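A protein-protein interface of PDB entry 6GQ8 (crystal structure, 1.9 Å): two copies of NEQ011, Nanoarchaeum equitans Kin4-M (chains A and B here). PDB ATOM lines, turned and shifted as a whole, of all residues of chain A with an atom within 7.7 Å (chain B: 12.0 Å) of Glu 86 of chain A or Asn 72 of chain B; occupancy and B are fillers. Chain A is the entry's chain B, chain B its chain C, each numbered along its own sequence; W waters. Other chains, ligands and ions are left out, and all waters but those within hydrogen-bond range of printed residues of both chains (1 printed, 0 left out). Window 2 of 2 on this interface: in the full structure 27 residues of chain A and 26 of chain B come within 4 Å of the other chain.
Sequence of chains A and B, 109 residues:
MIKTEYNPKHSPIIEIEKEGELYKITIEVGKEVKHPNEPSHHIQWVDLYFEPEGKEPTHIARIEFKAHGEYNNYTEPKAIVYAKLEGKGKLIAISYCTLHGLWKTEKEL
Hydrophobic or aromatic side chains of chain B within 4 Å of the printed part of chain A: Tyr 71.
Of the 16 printed residues of chain A, 7 touch a printed residue of chain B.
Printed residues of chain A that touch a printed residue of chain B: Phe 50, Lys 55, Thr 58, Ala 83, Lys 84, Leu 85 and Glu 86.
Hydrophobic or aromatic side chains of chain A that line the printed part of chain B: Phe 50, Ala 83 and Leu 85.
Along chain A the printed residues that touch a printed residue of chain B span positions 50 to 86.
Among the printed residues, no Asp or Glu carboxylate lies within 4 Å of a Lys or Arg side-chain nitrogen of the other chain.
The side-chain amide oxygen of Asn 73 of chain B is in hydrogen-bond range of the backbone NH of Glu 86 of chain A.
The backbone carbonyl oxygen (O) of Tyr 74 of chain B is in hydrogen-bond range of the backbone NH (N) of Lys 84 of chain A.
OE1 of Glu 86 of chain A sits at hydrogen-bond distance from ND2 of Asn 72 of chain B, 2.7 Å away.
Water W1 lies within hydrogen-bond range of O of Tyr 71 of chain B, O of Glu 86 of chain A and ND2 of Asn 73 of chain B.
Glu 86 of chain A touches just these residues of chain B: Tyr 71 (3.7 Å), Asn 72 (2.7 Å) and Asn 73 (3.0 Å).
Of chain A, only Glu 86 (2.7 Å) comes within 4 Å of Asn 72 of chain B.
Of chain B, only Asn 73 and Tyr 74 come within 4 Å of Lys 84 of chain A.
Leu 85 of chain A touches one residue of chain B.
Of the printed residues of chain B, Lys 55 of chain A touches Tyr 71.
Printed residues of chain B within 4 Å of Ala 83 of chain A: Tyr 74 (3.1 Å).
Printed residues of chain B within 4 Å of Phe 50 of chain A: Asn 73 (3.8 Å).
Glu 70 of chain B touches none of the printed residues of chain A.
The nearest printed residue of chain A that does not touch Tyr 74 of chain B is Leu 85 of chain A (5.2 Å).
No position is printed for both chains.
Phe 50 of chain A touches Asn 73 of chain B (CD2 to OD1, 3.8 Å).
CD of Lys 55 of chain A touches CD1 of Tyr 71 of chain B, 3.7 Å away.
Tyr 71 of chain B touches Thr 58 of chain A (CD2 to OG1, 3.4 Å).
Asn 73 of chain B touches Thr 58 of chain A.
Ala 83 of chain A touches Tyr 74 of chain B (CA to O, 3.1 Å).
Lys 84 of chain A touches Asn 73 of chain B (O to CA, 3.3 Å).
Leu 85 of chain A touches Asn 73 of chain B.
Tyr 71 of chain B touches Glu 86 of chain A (O to OE1, 3.7 Å).
The backbone carbonyl oxygen (O) of Glu 70 of chain B lies within hydrogen-bond range of the side-chain amide nitrogen (ND2) of Asn 73 of chain B.
The backbone carbonyl oxygen of Ala 83 of chain A sits at hydrogen-bond distance from the backbone NH of Tyr 23 of chain A.
The backbone carbonyl oxygen (O) of Phe 50 of chain A lies within hydrogen-bond range of the backbone NH (N) of Thr 58 of chain A.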
ATOM      1  N   GLU A  21      13.699   5.938  -2.599  1.00  0.00           N
ATOM      2  CA  GLU A  21      14.549   4.848  -3.058  1.00  0.00           C
ATOM      3  C   GLU A  21      15.200   5.141  -4.402  1.00  0.00           C
ATOM      4  O   GLU A  21      16.117   4.415  -4.803  1.00  0.00           O
ATOM      5  CB  GLU A  21      13.739   3.554  -3.150  1.00  0.00           C
ATOM      6  CG  GLU A  21      13.261   3.030  -1.805  1.00  0.00           C
ATOM      7  CD  GLU A  21      12.439   1.763  -1.934  1.00  0.00           C
ATOM      8  OE1 GLU A  21      12.739   0.949  -2.832  1.00  0.00           O
ATOM      9  OE2 GLU A  21      11.491   1.584  -1.139  1.00  0.00           O
ATOM     10  N   TYR A  23      17.238   7.363  -7.345  1.00  0.00           N
ATOM     11  CA  TYR A  23      18.134   8.439  -7.739  1.00  0.00           C
ATOM     12  C   TYR A  23      17.553   9.107  -8.978  1.00  0.00           C
ATOM     13  O   TYR A  23      17.273   8.433  -9.974  1.00  0.00           O
ATOM     14  CB  TYR A  23      19.536   7.911  -8.038  1.00  0.00           C
ATOM     15  CG  TYR A  23      20.327   7.490  -6.823  1.00  0.00           C
ATOM     16  CD1 TYR A  23      21.129   8.399  -6.147  1.00  0.00           C
ATOM     17  CD2 TYR A  23      20.286   6.183  -6.362  1.00  0.00           C
ATOM     18  CE1 TYR A  23      21.861   8.020  -5.039  1.00  0.00           C
ATOM     19  CE2 TYR A  23      21.014   5.794  -5.254  1.00  0.00           C
ATOM     20  CZ  TYR A  23      21.801   6.719  -4.598  1.00  0.00           C
ATOM     21  OH  TYR A  23      22.530   6.342  -3.493  1.00  0.00           O
ATOM     22  N   PHE A  50      26.579   2.975 -13.965  1.00  0.00           N
ATOM     23  CA  PHE A  50      26.901   3.036 -12.547  1.00  0.00           C
ATOM     24  C   PHE A  50      27.963   1.986 -12.272  1.00  0.00           C
ATOM     25  O   PHE A  50      27.757   0.802 -12.557  1.00  0.00           O
ATOM     26  CB  PHE A  50      25.665   2.805 -11.675  1.00  0.00           C
ATOM     27  CG  PHE A  50      25.975   2.712 -10.207  1.00  0.00           C
ATOM     28  CD1 PHE A  50      26.620   3.748  -9.555  1.00  0.00           C
ATOM     29  CD2 PHE A  50      25.620   1.586  -9.480  1.00  0.00           C
ATOM     30  CE1 PHE A  50      26.908   3.664  -8.203  1.00  0.00           C
ATOM     31  CE2 PHE A  50      25.903   1.496  -8.131  1.00  0.00           C
ATOM     32  CZ  PHE A  50      26.548   2.535  -7.491  1.00  0.00           C
ATOM     33  N   GLU A  51      29.107   2.424 -11.751  1.00  0.00           N
ATOM     34  CA  GLU A  51      30.196   1.522 -11.391  1.00  0.00           C
ATOM     35  C   GLU A  51      30.318   1.484  -9.875  1.00  0.00           C
ATOM     36  O   GLU A  51      31.000   2.332  -9.281  1.00  0.00           O
ATOM     37  CB  GLU A  51      31.516   1.960 -12.032  1.00  0.00           C
ATOM     38  CG  GLU A  51      32.655   0.976 -11.803  1.00  0.00           C
ATOM     39  CD  GLU A  51      33.955   1.425 -12.437  1.00  0.00           C
ATOM     40  OE1 GLU A  51      33.905   2.121 -13.471  1.00  0.00           O
ATOM     41  OE2 GLU A  51      35.028   1.084 -11.897  1.00  0.00           O
ATOM     42  N   PRO A  52      29.662   0.542  -9.201  1.00  0.00           N
ATOM     43  CA  PRO A  52      29.846   0.421  -7.750  1.00  0.00           C
ATOM     44  C   PRO A  52      31.289   0.067  -7.427  1.00  0.00           C
ATOM     45  O   PRO A  52      31.966  -0.624  -8.190  1.00  0.00           O
ATOM     46  CB  PRO A  52      28.880  -0.704  -7.356  1.00  0.00           C
ATOM     47  CG  PRO A  52      28.611  -1.451  -8.618  1.00  0.00           C
ATOM     48  CD  PRO A  52      28.738  -0.471  -9.739  1.00  0.00           C
ATOM     49  N   GLU A  53      31.766   0.586  -6.296  1.00  0.00           N
ATOM     50  CA  GLU A  53      33.160   0.407  -5.913  1.00  0.00           C
ATOM     51  C   GLU A  53      33.519  -1.073  -5.856  1.00  0.00           C
ATOM     52  O   GLU A  53      32.886  -1.851  -5.136  1.00  0.00           O
ATOM     53  CB  GLU A  53      33.421   1.071  -4.560  1.00  0.00           C
ATOM     54  CG  GLU A  53      32.370   0.766  -3.498  1.00  0.00           C
ATOM     55  CD  GLU A  53      32.517   1.623  -2.255  1.00  0.00           C
ATOM     56  OE1 GLU A  53      32.965   2.784  -2.375  1.00  0.00           O
ATOM     57  OE2 GLU A  53      32.188   1.134  -1.154  1.00  0.00           O
ATOM     58  N   LYS A  55      33.324  -3.232  -8.427  1.00  0.00           N
ATOM     59  CA  LYS A  55      32.525  -4.058  -9.323  1.00  0.00           C
ATOM     60  C   LYS A  55      32.639  -3.542 -10.753  1.00  0.00           C
ATOM     61  O   LYS A  55      33.313  -2.546 -11.035  1.00  0.00           O
ATOM     62  CB  LYS A  55      31.054  -4.101  -8.888  1.00  0.00           C
ATOM     63  CG  LYS A  55      30.816  -4.684  -7.506  1.00  0.00           C
ATOM     64  CD  LYS A  55      29.334  -4.950  -7.280  1.00  0.00           C
ATOM     65  CE  LYS A  55      29.035  -5.241  -5.817  1.00  0.00           C
ATOM     66  NZ  LYS A  55      29.122  -4.014  -4.978  1.00  0.00           N
ATOM     67  N   THR A  58      27.722  -1.105 -14.573  1.00  0.00           N
ATOM     68  CA  THR A  58      26.387  -1.554 -14.946  1.00  0.00           C
ATOM     69  C   THR A  58      25.722  -0.481 -15.796  1.00  0.00           C
ATOM     70  O   THR A  58      25.633   0.680 -15.381  1.00  0.00           O
ATOM     71  CB  THR A  58      25.528  -1.844 -13.714  1.00  0.00           C
ATOM     72  OG1 THR A  58      26.072  -2.955 -12.987  1.00  0.00           O
ATOM     73  CG2 THR A  58      24.095  -2.156 -14.126  1.00  0.00           C
ATOM     74  N   ALA A  83      16.716   5.614 -11.241  1.00  0.00           N
ATOM     75  CA  ALA A  83      17.233   4.280 -10.980  1.00  0.00           C
ATOM     76  C   ALA A  83      17.360   4.043  -9.484  1.00  0.00           C
ATOM     77  O   ALA A  83      17.583   4.976  -8.705  1.00  0.00           O
ATOM     78  CB  ALA A  83      18.590   4.067 -11.660  1.00  0.00           C
ATOM     79  N   LYS A  84      17.187   2.783  -9.090  1.00  0.00           N
ATOM     80  CA  LYS A  84      17.604   2.316  -7.775  1.00  0.00           C
ATOM     81  C   LYS A  84      19.014   1.758  -7.909  1.00  0.00           C
ATOM     82  O   LYS A  84      19.262   0.871  -8.735  1.00  0.00           O
ATOM     83  CB  LYS A  84      16.655   1.260  -7.205  1.00  0.00           C
ATOM     84  CG  LYS A  84      15.240   1.752  -6.966  1.00  0.00           C
ATOM     85  CD  LYS A  84      14.378   0.706  -6.275  1.00  0.00           C
ATOM     86  CE  LYS A  84      13.842  -0.331  -7.242  1.00  0.00           C
ATOM     87  NZ  LYS A  84      12.945  -1.289  -6.533  1.00  0.00           N
ATOM     88  N   LEU A  85      19.943   2.307  -7.135  1.00  0.00           N
ATOM     89  CA  LEU A  85      21.345   1.926  -7.195  1.00  0.00           C
ATOM     90  C   LEU A  85      21.779   1.456  -5.815  1.00  0.00           C
ATOM     91  O   LEU A  85      21.538   2.144  -4.818  1.00  0.00           O
ATOM     92  CB  LEU A  85      22.208   3.100  -7.661  1.00  0.00           C
ATOM     93  CG  LEU A  85      21.772   3.743  -8.979  1.00  0.00           C
ATOM     94  CD1 LEU A  85      22.621   4.960  -9.280  1.00  0.00           C
ATOM     95  CD2 LEU A  85      21.841   2.740 -10.121  1.00  0.00           C
ATOM     96  N   GLU A  86      22.411   0.288  -5.756  1.00  0.00           N
ATOM     97  CA  GLU A  86      22.826  -0.306  -4.491  1.00  0.00           C
ATOM     98  C   GLU A  86      24.295   0.001  -4.226  1.00  0.00           C
ATOM     99  O   GLU A  86      25.147  -0.207  -5.096  1.00  0.00           O
ATOM    100  CB  GLU A  86      22.599  -1.820  -4.484  1.00  0.00           C
ATOM    101  CG  GLU A  86      22.915  -2.474  -3.142  1.00  0.00           C
ATOM    102  CD  GLU A  86      22.771  -3.986  -3.173  1.00  0.00           C
ATOM    103  OE1 GLU A  86      23.531  -4.634  -3.923  1.00  0.00           O
ATOM    104  OE2 GLU A  86      21.917  -4.526  -2.440  1.00  0.00           O
ATOM    105  N   GLY A  87      24.580   0.512  -3.031  1.00  0.00           N
ATOM    106  CA  GLY A  87      25.946   0.749  -2.617  1.00  0.00           C
ATOM    107  C   GLY A  87      26.486   2.078  -3.101  1.00  0.00           C
ATOM    108  O   GLY A  87      25.802   2.890  -3.728  1.00  0.00           O
ATOM    109  N   LYS A  88      27.758   2.298  -2.796  1.00  0.00           N
ATOM    110  CA  LYS A  88      28.450   3.507  -3.208  1.00  0.00           C
ATOM    111  C   LYS A  88      29.227   3.257  -4.495  1.00  0.00           C
ATOM    112  O   LYS A  88      29.556   2.121  -4.844  1.00  0.00           O
ATOM    113  CB  LYS A  88      29.394   3.987  -2.105  1.00  0.00           C
ATOM    114  CG  LYS A  88      28.676   4.455  -0.846  1.00  0.00           C
ATOM    115  CD  LYS A  88      29.641   5.068   0.159  1.00  0.00           C
ATOM    116  CE  LYS A  88      28.905   5.605   1.379  1.00  0.00           C
ATOM    117  NZ  LYS A  88      29.848   6.117   2.411  1.00  0.00           N
ATOM    118  N   GLY A  89      29.520   4.346  -5.197  1.00  0.00           N
ATOM    119  CA  GLY A  89      30.211   4.246  -6.468  1.00  0.00           C
ATOM    120  C   GLY A  89      30.167   5.577  -7.191  1.00  0.00           C
ATOM    121  O   GLY A  89      29.964   6.624  -6.575  1.00  0.00           O
ATOM    122  N   LEU A 109      28.748   8.953  -6.435  1.00  0.00           N
ATOM    123  CA  LEU A 109      27.376   8.813  -5.970  1.00  0.00           C
ATOM    124  C   LEU A 109      27.257   9.249  -4.514  1.00  0.00           C
ATOM    125  O   LEU A 109      28.067   8.867  -3.667  1.00  0.00           O
ATOM    126  CB  LEU A 109      26.894   7.370  -6.131  1.00  0.00           C
ATOM    127  CG  LEU A 109      25.383   7.167  -6.027  1.00  0.00           C
ATOM    128  CD1 LEU A 109      24.684   7.893  -7.165  1.00  0.00           C
ATOM    129  CD2 LEU A 109      25.024   5.691  -6.019  1.00  0.00           C
ATOM    130  OXT LEU A 109      26.347   9.994  -4.150  1.00  0.00           O
ATOM    131  N   ASN B  37       9.613  -5.066 -12.429  1.00  0.00           N
ATOM    132  CA  ASN B  37      10.931  -4.738 -12.985  1.00  0.00           C
ATOM    133  C   ASN B  37      11.869  -5.880 -12.604  1.00  0.00           C
ATOM    134  O   ASN B  37      12.630  -5.787 -11.638  1.00  0.00           O
ATOM    135  CB  ASN B  37      11.433  -3.378 -12.482  1.00  0.00           C
ATOM    136  CG  ASN B  37      12.576  -2.832 -13.322  1.00  0.00           C
ATOM    137  OD1 ASN B  37      13.262  -3.578 -14.021  1.00  0.00           O
ATOM    138  ND2 ASN B  37      12.782  -1.521 -13.259  1.00  0.00           N
ATOM    139  N   GLU B  38      11.822  -6.949 -13.385  1.00  0.00           N
ATOM    140  CA  GLU B  38      12.529  -8.192 -13.121  1.00  0.00           C
ATOM    141  C   GLU B  38      13.329  -8.574 -14.353  1.00  0.00           C
ATOM    142  O   GLU B  38      13.055  -8.087 -15.456  1.00  0.00           O
ATOM    143  CB  GLU B  38      11.546  -9.322 -12.775  1.00  0.00           C
ATOM    144  CG  GLU B  38      10.560  -8.987 -11.668  1.00  0.00           C
ATOM    145  CD  GLU B  38       9.377  -9.939 -11.634  1.00  0.00           C
ATOM    146  OE1 GLU B  38       9.287 -10.817 -12.518  1.00  0.00           O
ATOM    147  OE2 GLU B  38       8.531  -9.804 -10.726  1.00  0.00           O
ATOM    148  N   PRO B  39      14.341  -9.437 -14.201  1.00  0.00           N
ATOM    149  CA  PRO B  39      15.118  -9.849 -15.382  1.00  0.00           C
ATOM    150  C   PRO B  39      14.261 -10.433 -16.493  1.00  0.00           C
ATOM    151  O   PRO B  39      14.515 -10.157 -17.673  1.00  0.00           O
ATOM    152  CB  PRO B  39      16.101 -10.874 -14.804  1.00  0.00           C
ATOM    153  CG  PRO B  39      16.287 -10.435 -13.389  1.00  0.00           C
ATOM    154  CD  PRO B  39      14.943  -9.928 -12.947  1.00  0.00           C
ATOM    155  N   LYS B  66      17.950   0.108 -18.835  1.00  0.00           N
ATOM    156  CA  LYS B  66      18.902  -0.974 -19.065  1.00  0.00           C
ATOM    157  C   LYS B  66      19.109  -1.909 -17.881  1.00  0.00           C
ATOM    158  O   LYS B  66      19.479  -3.067 -18.093  1.00  0.00           O
ATOM    159  CB  LYS B  66      20.263  -0.400 -19.470  1.00  0.00           C
ATOM    160  CG  LYS B  66      20.298   0.220 -20.851  1.00  0.00           C
ATOM    161  CD  LYS B  66      19.993  -0.829 -21.894  1.00  0.00           C
ATOM    162  CE  LYS B  66      20.712  -0.542 -23.195  1.00  0.00           C
ATOM    163  NZ  LYS B  66      20.450  -1.628 -24.168  1.00  0.00           N
ATOM    164  N   ALA B  67      18.904  -1.452 -16.650  1.00  0.00           N
ATOM    165  CA  ALA B  67      19.192  -2.258 -15.470  1.00  0.00           C
ATOM    166  C   ALA B  67      17.904  -2.856 -14.921  1.00  0.00           C
ATOM    167  O   ALA B  67      16.905  -2.147 -14.755  1.00  0.00           O
ATOM    168  CB  ALA B  67      19.891  -1.423 -14.395  1.00  0.00           C
ATOM    169  N   HIS B  68      17.932  -4.157 -14.637  1.00  0.00           N
ATOM    170  CA  HIS B  68      16.764  -4.889 -14.151  1.00  0.00           C
ATOM    171  C   HIS B  68      17.184  -5.939 -13.133  1.00  0.00           C
ATOM    172  O   HIS B  68      16.672  -7.064 -13.123  1.00  0.00           O
ATOM    173  CB  HIS B  68      15.993  -5.534 -15.303  1.00  0.00           C
ATOM    174  CG  HIS B  68      15.676  -4.588 -16.418  1.00  0.00           C
ATOM    175  ND1 HIS B  68      14.708  -3.614 -16.314  1.00  0.00           N
ATOM    176  CD2 HIS B  68      16.207  -4.463 -17.658  1.00  0.00           C
ATOM    177  CE1 HIS B  68      14.655  -2.927 -17.442  1.00  0.00           C
ATOM    178  NE2 HIS B  68      15.552  -3.424 -18.276  1.00  0.00           N
ATOM    179  N   GLY B  69      18.122  -5.585 -12.261  1.00  0.00           N
ATOM    180  CA  GLY B  69      18.571  -6.472 -11.203  1.00  0.00           C
ATOM    181  C   GLY B  69      20.058  -6.740 -11.189  1.00  0.00           C
ATOM    182  O   GLY B  69      20.558  -7.307 -10.205  1.00  0.00           O
ATOM    183  N   GLU B  70      20.789  -6.373 -12.241  1.00  0.00           N
ATOM    184  CA  GLU B  70      22.232  -6.574 -12.266  1.00  0.00           C
ATOM    185  C   GLU B  70      22.874  -5.839 -11.099  1.00  0.00           C
ATOM    186  O   GLU B  70      22.810  -4.607 -11.020  1.00  0.00           O
ATOM    187  CB  GLU B  70      22.813  -6.085 -13.593  1.00  0.00           C
ATOM    188  CG  GLU B  70      22.377  -6.880 -14.813  1.00  0.00           C
ATOM    189  CD  GLU B  70      21.081  -6.374 -15.417  1.00  0.00           C
ATOM    190  OE1 GLU B  70      20.403  -5.549 -14.772  1.00  0.00           O
ATOM    191  OE2 GLU B  70      20.746  -6.794 -16.547  1.00  0.00           O
ATOM    192  N   TYR B  71      23.492  -6.600 -10.197  1.00  0.00           N
ATOM    193  CA  TYR B  71      24.075  -6.058  -8.969  1.00  0.00           C
ATOM    194  C   TYR B  71      23.057  -5.228  -8.188  1.00  0.00           C
ATOM    195  O   TYR B  71      23.402  -4.223  -7.561  1.00  0.00           O
ATOM    196  CB  TYR B  71      25.343  -5.255  -9.271  1.00  0.00           C
ATOM    197  CG  TYR B  71      26.401  -6.067  -9.991  1.00  0.00           C
ATOM    198  CD1 TYR B  71      27.125  -7.044  -9.323  1.00  0.00           C
ATOM    199  CD2 TYR B  71      26.669  -5.863 -11.341  1.00  0.00           C
ATOM    200  CE1 TYR B  71      28.088  -7.795  -9.973  1.00  0.00           C
ATOM    201  CE2 TYR B  71      27.632  -6.610 -12.000  1.00  0.00           C
ATOM    202  CZ  TYR B  71      28.338  -7.573 -11.310  1.00  0.00           C
ATOM    203  OH  TYR B  71      29.296  -8.321 -11.954  1.00  0.00           O
ATOM    204  N   ASN B  72      21.791  -5.656  -8.239  1.00  0.00           N
ATOM    205  CA  ASN B  72      20.685  -5.038  -7.499  1.00  0.00           C
ATOM    206  C   ASN B  72      20.421  -3.602  -7.944  1.00  0.00           C
ATOM    207  O   ASN B  72      19.966  -2.769  -7.156  1.00  0.00           O
ATOM    208  CB  ASN B  72      20.929  -5.103  -5.990  1.00  0.00           C
ATOM    209  CG  ASN B  72      21.051  -6.528  -5.490  1.00  0.00           C
ATOM    210  OD1 ASN B  72      20.259  -7.396  -5.861  1.00  0.00           O
ATOM    211  ND2 ASN B  72      22.052  -6.780  -4.656  1.00  0.00           N
ATOM    212  N   ASN B  73      20.695  -3.307  -9.210  1.00  0.00           N
ATOM    213  CA  ASN B  73      20.402  -2.013  -9.810  1.00  0.00           C
ATOM    214  C   ASN B  73      19.198  -2.128 -10.738  1.00  0.00           C
ATOM    215  O   ASN B  73      19.067  -3.108 -11.480  1.00  0.00           O
ATOM    216  CB  ASN B  73      21.619  -1.489 -10.575  1.00  0.00           C
ATOM    217  CG  ASN B  73      22.826  -1.293  -9.676  1.00  0.00           C
ATOM    218  OD1 ASN B  73      22.732  -0.662  -8.625  1.00  0.00           O
ATOM    219  ND2 ASN B  73      23.961  -1.851 -10.076  1.00  0.00           N
ATOM    220  N   TYR B  74      18.310  -1.133 -10.676  1.00  0.00           N
ATOM    221  CA  TYR B  74      17.061  -1.136 -11.432  1.00  0.00           C
ATOM    222  C   TYR B  74      16.804   0.241 -12.020  1.00  0.00           C
ATOM    223  O   TYR B  74      16.742   1.225 -11.280  1.00  0.00           O
ATOM    224  CB  TYR B  74      15.871  -1.525 -10.546  1.00  0.00           C
ATOM    225  CG  TYR B  74      15.957  -2.911  -9.965  1.00  0.00           C
ATOM    226  CD1 TYR B  74      15.361  -3.987 -10.607  1.00  0.00           C
ATOM    227  CD2 TYR B  74      16.627  -3.147  -8.771  1.00  0.00           C
ATOM    228  CE1 TYR B  74      15.433  -5.259 -10.081  1.00  0.00           C
ATOM    229  CE2 TYR B  74      16.706  -4.420  -8.239  1.00  0.00           C
ATOM    230  CZ  TYR B  74      16.107  -5.469  -8.899  1.00  0.00           C
ATOM    231  OH  TYR B  74      16.180  -6.736  -8.375  1.00  0.00           O
ATOM    232  N   THR B  75      16.615   0.304 -13.336  1.00  0.00           N
ATOM    233  CA  THR B  75      16.209   1.538 -14.001  1.00  0.00           C
ATOM    234  C   THR B  75      14.687   1.576 -14.069  1.00  0.00           C
ATOM    235  O   THR B  75      14.065   0.690 -14.665  1.00  0.00           O
ATOM    236  CB  THR B  75      16.795   1.641 -15.410  1.00  0.00           C
ATOM    237  OG1 THR B  75      18.203   1.380 -15.373  1.00  0.00           O
ATOM    238  CG2 THR B  75      16.559   3.042 -15.981  1.00  0.00           C
ATOM    239  N   GLU B  76      14.091   2.588 -13.453  1.00  0.00           N
ATOM    240  CA  GLU B  76      12.643   2.714 -13.494  1.00  0.00           C
ATOM    241  C   GLU B  76      12.193   3.184 -14.875  1.00  0.00           C
ATOM    242  O   GLU B  76      12.877   3.992 -15.511  1.00  0.00           O
ATOM    243  CB  GLU B  76      12.156   3.685 -12.422  1.00  0.00           C
ATOM    244  CG  GLU B  76      12.148   3.081 -11.033  1.00  0.00           C
ATOM    245  CD  GLU B  76      11.207   1.898 -10.920  1.00  0.00           C
ATOM    246  OE1 GLU B  76       9.979   2.124 -10.858  1.00  0.00           O
ATOM    247  OE2 GLU B  76      11.693   0.747 -10.892  1.00  0.00           O
HETATM  248  O   HOH W   1      25.678  -2.420  -7.210  1.00  0.00           O
